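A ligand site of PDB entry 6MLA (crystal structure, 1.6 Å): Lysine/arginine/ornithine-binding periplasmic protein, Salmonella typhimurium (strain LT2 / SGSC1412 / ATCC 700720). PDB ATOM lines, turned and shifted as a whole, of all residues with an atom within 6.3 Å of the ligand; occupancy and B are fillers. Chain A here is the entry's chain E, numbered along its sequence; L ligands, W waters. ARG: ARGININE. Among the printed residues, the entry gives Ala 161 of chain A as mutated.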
ATOM      1  N   THR A  10       9.514  -7.380 -31.026  1.00  0.00           N
ATOM      2  CA  THR A  10       9.799  -7.641 -29.632  1.00  0.00           C
ATOM      3  C   THR A  10      10.437  -9.039 -29.479  1.00  0.00           C
ATOM      4  O   THR A  10      10.197  -9.951 -30.280  1.00  0.00           O
ATOM      5  CB  THR A  10       8.521  -7.512 -28.761  1.00  0.00           C
ATOM      6  OG1 THR A  10       8.873  -7.483 -27.373  1.00  0.00           O
ATOM      7  CG2 THR A  10       7.529  -8.656 -29.042  1.00  0.00           C
ATOM      8  N   ASP A  11      11.288  -9.182 -28.459  1.00  0.00           N
ATOM      9  CA  ASP A  11      11.929 -10.441 -28.110  1.00  0.00           C
ATOM     10  C   ASP A  11      11.129 -11.032 -26.983  1.00  0.00           C
ATOM     11  O   ASP A  11      11.210 -10.579 -25.844  1.00  0.00           O
ATOM     12  CB  ASP A  11      13.387 -10.194 -27.703  1.00  0.00           C
ATOM     13  CG  ASP A  11      14.030 -11.390 -27.028  1.00  0.00           C
ATOM     14  OD1 ASP A  11      13.515 -12.526 -27.128  1.00  0.00           O
ATOM     15  OD2 ASP A  11      15.085 -11.178 -26.396  1.00  0.00           O
ATOM     16  N   THR A  12      10.335 -12.041 -27.327  1.00  0.00           N
ATOM     17  CA  THR A  12       9.381 -12.645 -26.401  1.00  0.00           C
ATOM     18  C   THR A  12       9.994 -13.661 -25.431  1.00  0.00           C
ATOM     19  O   THR A  12       9.360 -14.678 -25.112  1.00  0.00           O
ATOM     20  CB  THR A  12       8.261 -13.332 -27.183  1.00  0.00           C
ATOM     21  OG1 THR A  12       8.823 -14.344 -28.025  1.00  0.00           O
ATOM     22  CG2 THR A  12       7.540 -12.296 -28.041  1.00  0.00           C
ATOM     23  N   THR A  13      11.199 -13.370 -24.954  1.00  0.00           N
ATOM     24  CA  THR A  13      11.892 -14.230 -24.012  1.00  0.00           C
ATOM     25  C   THR A  13      12.405 -13.433 -22.797  1.00  0.00           C
ATOM     26  O   THR A  13      13.458 -13.742 -22.229  1.00  0.00           O
ATOM     27  CB  THR A  13      13.072 -14.974 -24.686  1.00  0.00           C
ATOM     28  OG1 THR A  13      14.004 -14.020 -25.223  1.00  0.00           O
ATOM     29  CG2 THR A  13      12.578 -15.882 -25.832  1.00  0.00           C
ATOM     30  N   TYR A  14      11.659 -12.408 -22.395  1.00  0.00           N
ATOM     31  CA  TYR A  14      12.119 -11.515 -21.335  1.00  0.00           C
ATOM     32  C   TYR A  14      10.968 -11.164 -20.390  1.00  0.00           C
ATOM     33  O   TYR A  14      10.617  -9.993 -20.240  1.00  0.00           O
ATOM     34  CB  TYR A  14      12.719 -10.251 -21.940  1.00  0.00           C
ATOM     35  CG  TYR A  14      13.954  -9.673 -21.298  1.00  0.00           C
ATOM     36  CD1 TYR A  14      15.173 -10.340 -21.357  1.00  0.00           C
ATOM     37  CD2 TYR A  14      13.929  -8.424 -20.692  1.00  0.00           C
ATOM     38  CE1 TYR A  14      16.326  -9.776 -20.816  1.00  0.00           C
ATOM     39  CE2 TYR A  14      15.055  -7.868 -20.128  1.00  0.00           C
ATOM     40  CZ  TYR A  14      16.256  -8.546 -20.194  1.00  0.00           C
ATOM     41  OH  TYR A  14      17.397  -7.987 -19.646  1.00  0.00           O
ATOM     42  N   PHE A  17       8.327  -8.515 -19.158  1.00  0.00           N
ATOM     43  CA  PHE A  17       8.168  -7.419 -20.088  1.00  0.00           C
ATOM     44  C   PHE A  17       7.610  -7.930 -21.406  1.00  0.00           C
ATOM     45  O   PHE A  17       6.604  -7.401 -21.897  1.00  0.00           O
ATOM     46  CB  PHE A  17       9.506  -6.702 -20.252  1.00  0.00           C
ATOM     47  CG  PHE A  17      10.002  -6.064 -18.973  1.00  0.00           C
ATOM     48  CD1 PHE A  17       9.397  -4.915 -18.484  1.00  0.00           C
ATOM     49  CD2 PHE A  17      11.021  -6.644 -18.232  1.00  0.00           C
ATOM     50  CE1 PHE A  17       9.828  -4.304 -17.304  1.00  0.00           C
ATOM     51  CE2 PHE A  17      11.450  -6.047 -17.027  1.00  0.00           C
ATOM     52  CZ  PHE A  17      10.851  -4.874 -16.576  1.00  0.00           C
ATOM     53  N   SER A  18       8.200  -9.001 -21.928  1.00  0.00           N
ATOM     54  CA  SER A  18       7.754  -9.565 -23.191  1.00  0.00           C
ATOM     55  C   SER A  18       8.003 -11.065 -23.200  1.00  0.00           C
ATOM     56  O   SER A  18       9.146 -11.503 -23.100  1.00  0.00           O
ATOM     57  CB  SER A  18       8.479  -8.900 -24.358  1.00  0.00           C
ATOM     58  OG  SER A  18       8.152  -9.533 -25.592  1.00  0.00           O
ATOM     59  N   ASP A  30       5.611  -4.718 -21.665  1.00  0.00           N
ATOM     60  CA  ASP A  30       5.887  -4.099 -22.975  1.00  0.00           C
ATOM     61  C   ASP A  30       4.683  -4.237 -23.915  1.00  0.00           C
ATOM     62  O   ASP A  30       4.363  -3.315 -24.680  1.00  0.00           O
ATOM     63  CB  ASP A  30       7.093  -4.750 -23.640  1.00  0.00           C
ATOM     64  CG  ASP A  30       8.415  -4.236 -23.131  1.00  0.00           C
ATOM     65  OD1 ASP A  30       8.441  -3.263 -22.328  1.00  0.00           O
ATOM     66  OD2 ASP A  30       9.445  -4.822 -23.535  1.00  0.00           O
ATOM     67  N   PHE A  52      16.603 -10.799 -29.906  1.00  0.00           N
ATOM     68  CA  PHE A  52      16.861  -9.426 -29.513  1.00  0.00           C
ATOM     69  C   PHE A  52      17.860  -8.729 -30.454  1.00  0.00           C
ATOM     70  O   PHE A  52      17.637  -7.583 -30.842  1.00  0.00           O
ATOM     71  CB  PHE A  52      17.383  -9.367 -28.075  1.00  0.00           C
ATOM     72  CG  PHE A  52      17.594  -7.956 -27.589  1.00  0.00           C
ATOM     73  CD1 PHE A  52      16.515  -7.196 -27.172  1.00  0.00           C
ATOM     74  CD2 PHE A  52      18.862  -7.379 -27.606  1.00  0.00           C
ATOM     75  CE1 PHE A  52      16.683  -5.883 -26.752  1.00  0.00           C
ATOM     76  CE2 PHE A  52      19.036  -6.071 -27.180  1.00  0.00           C
ATOM     77  CZ  PHE A  52      17.954  -5.325 -26.737  1.00  0.00           C
ATOM     78  N   LEU A  55      16.581  -7.072 -33.733  1.00  0.00           N
ATOM     79  CA  LEU A  55      15.576  -5.998 -33.681  1.00  0.00           C
ATOM     80  C   LEU A  55      16.040  -4.699 -34.349  1.00  0.00           C
ATOM     81  O   LEU A  55      15.375  -4.169 -35.233  1.00  0.00           O
ATOM     82  CB  LEU A  55      15.194  -5.709 -32.227  1.00  0.00           C
ATOM     83  CG  LEU A  55      14.353  -6.797 -31.562  1.00  0.00           C
ATOM     84  CD1 LEU A  55      14.302  -6.601 -30.060  1.00  0.00           C
ATOM     85  CD2 LEU A  55      12.949  -6.822 -32.163  1.00  0.00           C
ATOM     86  N   ILE A  68       9.666  -2.524 -29.168  1.00  0.00           N
ATOM     87  CA  ILE A  68       9.341  -2.425 -27.753  1.00  0.00           C
ATOM     88  C   ILE A  68       9.774  -3.766 -27.162  1.00  0.00           C
ATOM     89  O   ILE A  68       9.110  -4.779 -27.348  1.00  0.00           O
ATOM     90  CB  ILE A  68       7.834  -2.128 -27.502  1.00  0.00           C
ATOM     91  CG1 ILE A  68       7.408  -0.872 -28.264  1.00  0.00           C
ATOM     92  CG2 ILE A  68       7.558  -1.964 -25.985  1.00  0.00           C
ATOM     93  CD1 ILE A  68       5.926  -0.512 -28.185  1.00  0.00           C
ATOM     94  N   SER A  69      10.938  -3.751 -26.526  1.00  0.00           N
ATOM     95  CA  SER A  69      11.560  -4.970 -26.058  1.00  0.00           C
ATOM     96  C   SER A  69      12.575  -4.628 -24.978  1.00  0.00           C
ATOM     97  O   SER A  69      13.728  -5.026 -25.075  1.00  0.00           O
ATOM     98  CB  SER A  69      12.224  -5.708 -27.226  1.00  0.00           C
ATOM     99  OG  SER A  69      12.459  -7.070 -26.906  1.00  0.00           O
ATOM    100  N   SER A  70      12.149  -3.889 -23.963  1.00  0.00           N
ATOM    101  CA  SER A  70      13.054  -3.381 -22.938  1.00  0.00           C
ATOM    102  C   SER A  70      14.320  -2.773 -23.559  1.00  0.00           C
ATOM    103  O   SER A  70      15.436  -3.017 -23.095  1.00  0.00           O
ATOM    104  CB  SER A  70      13.432  -4.510 -21.969  1.00  0.00           C
ATOM    105  OG  SER A  70      12.310  -4.988 -21.236  1.00  0.00           O
ATOM    106  N   LEU A  71      14.161  -1.966 -24.601  1.00  0.00           N
ATOM    107  CA  LEU A  71      15.302  -1.414 -25.334  1.00  0.00           C
ATOM    108  C   LEU A  71      15.897  -0.203 -24.655  1.00  0.00           C
ATOM    109  O   LEU A  71      15.314   0.885 -24.668  1.00  0.00           O
ATOM    110  CB  LEU A  71      14.882  -1.049 -26.741  1.00  0.00           C
ATOM    111  CG  LEU A  71      16.030  -0.694 -27.670  1.00  0.00           C
ATOM    112  CD1 LEU A  71      16.913  -1.913 -27.947  1.00  0.00           C
ATOM    113  CD2 LEU A  71      15.493  -0.126 -28.969  1.00  0.00           C
ATOM    114  N   SER A  72      17.066  -0.364 -24.056  1.00  0.00           N
ATOM    115  CA  SER A  72      17.680   0.699 -23.307  1.00  0.00           C
ATOM    116  C   SER A  72      18.066   1.891 -24.177  1.00  0.00           C
ATOM    117  O   SER A  72      18.640   1.742 -25.270  1.00  0.00           O
ATOM    118  CB  SER A  72      18.913   0.172 -22.582  1.00  0.00           C
ATOM    119  OG  SER A  72      18.524  -0.697 -21.543  1.00  0.00           O
ATOM    120  N   ILE A  73      17.754   3.079 -23.665  1.00  0.00           N
ATOM    121  CA  ILE A  73      18.088   4.315 -24.352  1.00  0.00           C
ATOM    122  C   ILE A  73      19.538   4.694 -24.061  1.00  0.00           C
ATOM    123  O   ILE A  73      19.833   5.230 -22.982  1.00  0.00           O
ATOM    124  CB  ILE A  73      17.154   5.469 -23.929  1.00  0.00           C
ATOM    125  CG1 ILE A  73      15.688   5.029 -24.019  1.00  0.00           C
ATOM    126  CG2 ILE A  73      17.463   6.715 -24.763  1.00  0.00           C
ATOM    127  CD1 ILE A  73      14.691   6.067 -23.488  1.00  0.00           C
ATOM    128  N   THR A  74      20.426   4.429 -25.014  1.00  0.00           N
ATOM    129  CA  THR A  74      21.859   4.671 -24.845  1.00  0.00           C
ATOM    130  C   THR A  74      22.417   5.660 -25.851  1.00  0.00           C
ATOM    131  O   THR A  74      21.867   5.822 -26.935  1.00  0.00           O
ATOM    132  CB  THR A  74      22.695   3.371 -24.980  1.00  0.00           C
ATOM    133  OG1 THR A  74      22.695   2.920 -26.348  1.00  0.00           O
ATOM    134  CG2 THR A  74      22.128   2.287 -24.080  1.00  0.00           C
ATOM    135  N   ARG A  77      23.242   3.890 -29.125  1.00  0.00           N
ATOM    136  CA  ARG A  77      22.095   3.570 -29.965  1.00  0.00           C
ATOM    137  C   ARG A  77      21.475   4.815 -30.559  1.00  0.00           C
ATOM    138  O   ARG A  77      20.905   4.766 -31.647  1.00  0.00           O
ATOM    139  CB  ARG A  77      21.057   2.783 -29.184  1.00  0.00           C
ATOM    140  CG  ARG A  77      21.414   1.315 -29.083  1.00  0.00           C
ATOM    141  CD  ARG A  77      20.516   0.622 -28.074  1.00  0.00           C
ATOM    142  NE  ARG A  77      20.869  -0.778 -27.879  1.00  0.00           N
ATOM    143  CZ  ARG A  77      20.430  -1.517 -26.872  1.00  0.00           C
ATOM    144  NH1 ARG A  77      19.639  -0.980 -25.962  1.00  0.00           N
ATOM    145  NH2 ARG A  77      20.791  -2.787 -26.760  1.00  0.00           N
ATOM    146  N   ALA A  90      15.573   0.376 -16.117  1.00  0.00           N
ATOM    147  CA  ALA A  90      16.047  -0.989 -16.257  1.00  0.00           C
ATOM    148  C   ALA A  90      17.497  -1.144 -15.824  1.00  0.00           C
ATOM    149  O   ALA A  90      18.389  -1.196 -16.674  1.00  0.00           O
ATOM    150  CB  ALA A  90      15.870  -1.474 -17.690  1.00  0.00           C
ATOM    151  N   LEU A 117      22.859 -11.688 -22.819  1.00  0.00           N
ATOM    152  CA  LEU A 117      22.056 -11.671 -24.047  1.00  0.00           C
ATOM    153  C   LEU A 117      22.796 -11.006 -25.194  1.00  0.00           C
ATOM    154  O   LEU A 117      23.267  -9.878 -25.069  1.00  0.00           O
ATOM    155  CB  LEU A 117      20.718 -10.962 -23.782  1.00  0.00           C
ATOM    156  CG  LEU A 117      19.826 -10.714 -25.001  1.00  0.00           C
ATOM    157  CD1 LEU A 117      19.269 -12.024 -25.510  1.00  0.00           C
ATOM    158  CD2 LEU A 117      18.708  -9.755 -24.632  1.00  0.00           C
ATOM    159  N   GLY A 119      23.670  -8.879 -28.244  1.00  0.00           N
ATOM    160  CA  GLY A 119      23.125  -7.618 -28.707  1.00  0.00           C
ATOM    161  C   GLY A 119      22.667  -6.690 -27.590  1.00  0.00           C
ATOM    162  O   GLY A 119      22.256  -5.567 -27.850  1.00  0.00           O
ATOM    163  N   SER A 120      22.791  -7.140 -26.346  1.00  0.00           N
ATOM    164  CA  SER A 120      22.304  -6.343 -25.216  1.00  0.00           C
ATOM    165  C   SER A 120      23.364  -5.396 -24.657  1.00  0.00           C
ATOM    166  O   SER A 120      24.552  -5.563 -24.913  1.00  0.00           O
ATOM    167  CB  SER A 120      21.819  -7.273 -24.105  1.00  0.00           C
ATOM    168  OG  SER A 120      22.914  -7.888 -23.453  1.00  0.00           O
ATOM    169  N   THR A 121      22.923  -4.406 -23.871  1.00  0.00           N
ATOM    170  CA  THR A 121      23.831  -3.528 -23.125  1.00  0.00           C
ATOM    171  C   THR A 121      24.646  -4.313 -22.103  1.00  0.00           C
ATOM    172  O   THR A 121      25.798  -3.973 -21.813  1.00  0.00           O
ATOM    173  CB  THR A 121      23.065  -2.437 -22.387  1.00  0.00           C
ATOM    174  OG1 THR A 121      22.045  -3.048 -21.615  1.00  0.00           O
ATOM    175  CG2 THR A 121      22.442  -1.460 -23.386  1.00  0.00           C
ATOM    176  N   GLN A 122      24.040  -5.365 -21.555  1.00  0.00           N
ATOM    177  CA  GLN A 122      24.733  -6.225 -20.613  1.00  0.00           C
ATOM    178  C   GLN A 122      25.895  -6.929 -21.298  1.00  0.00           C
ATOM    179  O   GLN A 122      26.970  -7.044 -20.707  1.00  0.00           O
ATOM    180  CB  GLN A 122      23.770  -7.228 -19.995  1.00  0.00           C
ATOM    181  CG  GLN A 122      22.771  -6.604 -19.027  1.00  0.00           C
ATOM    182  CD  GLN A 122      21.514  -6.088 -19.715  1.00  0.00           C
ATOM    183  OE1 GLN A 122      21.257  -6.353 -20.881  1.00  0.00           O
ATOM    184  NE2 GLN A 122      20.704  -5.330 -18.968  1.00  0.00           N
ATOM    185  N   GLN A 143      17.216 -14.869 -23.692  1.00  0.00           N
ATOM    186  CA  GLN A 143      17.415 -14.929 -22.266  1.00  0.00           C
ATOM    187  C   GLN A 143      16.962 -16.278 -21.683  1.00  0.00           C
ATOM    188  O   GLN A 143      17.435 -16.692 -20.635  1.00  0.00           O
ATOM    189  CB  GLN A 143      16.682 -13.768 -21.591  1.00  0.00           C
ATOM    190  CG  GLN A 143      16.881 -13.660 -20.087  1.00  0.00           C
ATOM    191  CD  GLN A 143      18.270 -13.210 -19.687  1.00  0.00           C
ATOM    192  OE1 GLN A 143      18.902 -12.403 -20.369  1.00  0.00           O
ATOM    193  NE2 GLN A 143      18.764 -13.738 -18.556  1.00  0.00           N
ATOM    194  N   ALA A 161      18.626  -7.551 -17.038  1.00  0.00           N
ATOM    195  CA  ALA A 161      17.860  -6.580 -16.238  1.00  0.00           C
ATOM    196  C   ALA A 161      17.464  -7.153 -14.867  1.00  0.00           C
ATOM    197  O   ALA A 161      16.962  -8.295 -14.780  1.00  0.00           O
ATOM    198  CB  ALA A 161      16.623  -6.136 -16.987  1.00  0.00           C
ATOM    199  N   THR A 195      14.306   2.515 -20.716  1.00  0.00           N
ATOM    200  CA  THR A 195      14.012   1.888 -22.003  1.00  0.00           C
ATOM    201  C   THR A 195      13.059   2.786 -22.759  1.00  0.00           C
ATOM    202  O   THR A 195      12.406   3.642 -22.157  1.00  0.00           O
ATOM    203  CB  THR A 195      13.401   0.493 -21.839  1.00  0.00           C
ATOM    204  OG1 THR A 195      12.150   0.610 -21.163  1.00  0.00           O
ATOM    205  CG2 THR A 195      14.352  -0.419 -21.057  1.00  0.00           C
HETATM  206  N   ARG L   1      17.825  -3.559 -21.753  1.00  0.00           N
HETATM  207  CA  ARG L   1      18.835  -4.363 -22.433  1.00  0.00           C
HETATM  208  C   ARG L   1      19.232  -3.734 -23.749  1.00  0.00           C
HETATM  209  O   ARG L   1      18.595  -2.806 -24.218  1.00  0.00           O
HETATM  210  CB  ARG L   1      18.312  -5.794 -22.658  1.00  0.00           C
HETATM  211  CG  ARG L   1      16.900  -5.854 -23.229  1.00  0.00           C
HETATM  212  CD  ARG L   1      16.409  -7.294 -23.482  1.00  0.00           C
HETATM  213  NE  ARG L   1      14.994  -7.332 -23.895  1.00  0.00           N
HETATM  214  CZ  ARG L   1      14.391  -8.403 -24.421  1.00  0.00           C
HETATM  215  NH1 ARG L   1      15.069  -9.527 -24.616  1.00  0.00           N
HETATM  216  NH2 ARG L   1      13.090  -8.347 -24.763  1.00  0.00           N
HETATM  217  OXT ARG L   1      20.217  -4.132 -24.392  1.00  0.00           O
HETATM  218  O   HOH W   1      15.820 -12.602 -24.434  1.00  0.00           O
HETATM  219  O   HOH W   2      18.428  -3.479 -19.040  1.00  0.00           O
HETATM  220  O   HOH W   3      11.175  -6.931 -22.976  1.00  0.00           O
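OH of Tyr 14 is in hydrogen-bond range of N of Ala 161, 2.9 Å away.
The backbone carbonyl oxygen (O) of Ser 72 lies within hydrogen-bond range of the guanidinium group (NH1) of Arg 77, 3.0 Å away.
O of Asp 11 sits at hydrogen-bond distance from OG of Ser 18, 3.2 Å away.
The side-chain carboxylate (OD1) of Asp 11 sits at hydrogen-bond distance from the side-chain hydroxyl (OG1) of Thr 13.
The side-chain hydroxyl of Ser 120 sits close to the backbone NH of Gln 122.
N of Arg 77 sits at hydrogen-bond distance from OG1 of Thr 74, at 3.0 Å.
The guanidinium group (NH2) of Arg 77 is in hydrogen-bond range of the backbone carbonyl oxygen (O) of Gly 119 (3.3 Å).
The backbone NH of Asp 11 is in hydrogen-bond range of the side-chain hydroxyl of Ser 69 (2.9 Å).
Tyr 14 touches the ligand.
CZ of Phe 52 touches OXT of the ligand, at 3.5 Å.
CA of Leu 71 touches O of the ligand (3.7 Å).
Leu 117 touches the ligand.
Ser 120 touches the ligand (CA to OXT, 3.2 Å).
OE1 of Gln 122 touches CB of the ligand, 3.5 Å away.
Of the 27 residues printed, 12 come within 4 Å of the ligand.
Along chain A the residues within 4 Å of the ligand span positions 11 to 122.
The backbone carbonyl oxygen (O) of Asp 11 is in hydrogen-bond range of a nitrogen (NH2) of the ligand (3.1 Å).
The backbone carbonyl oxygen (O) of Ser 69 sits at hydrogen-bond distance from a nitrogen (NE) of the ligand.
NH1 of Arg 77 is in salt-bridge range of O of the ligand, 2.7 Å away.
An oxygen (O) of the ligand lies within hydrogen-bond range of the backbone NH (N) of Ser 72 (2.9 Å).
OG of Ser 69 lies within hydrogen-bond range of NH2 of the ligand (2.6 Å).
OG1 of Thr 121 lies within hydrogen-bond range of OXT of the ligand, 3.5 Å away.
OG of Ser 72 is in hydrogen-bond range of N of the ligand.
O of Ser 70 lies within hydrogen-bond range of N of the ligand (2.8 Å).
OD2 of Asp 11 lies within salt-bridge range of NH1 of the ligand, 2.4 Å away.
N of Thr 121 lies within hydrogen-bond range of OXT of the ligand (2.8 Å).
Water W2 lies within hydrogen-bond range of N of the ligand (2.8 Å), NE2 of Gln 122 (2.9 Å) and O of Ala 90 (3.3 Å).
Water W3 lies within hydrogen-bond range of OD2 of Asp 30 (2.8 Å), OG of Ser 70 (2.8 Å) and NH2 of the ligand (3.0 Å).
Water W1 lies within hydrogen-bond range of the side-chain hydroxyl of Thr 13 (2.4 Å), the side-chain carboxylate of Asp 11 (2.5 Å), the backbone NH of Gln 143 (2.8 Å) and a nitrogen (NH1) of the ligand (3.2 Å).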
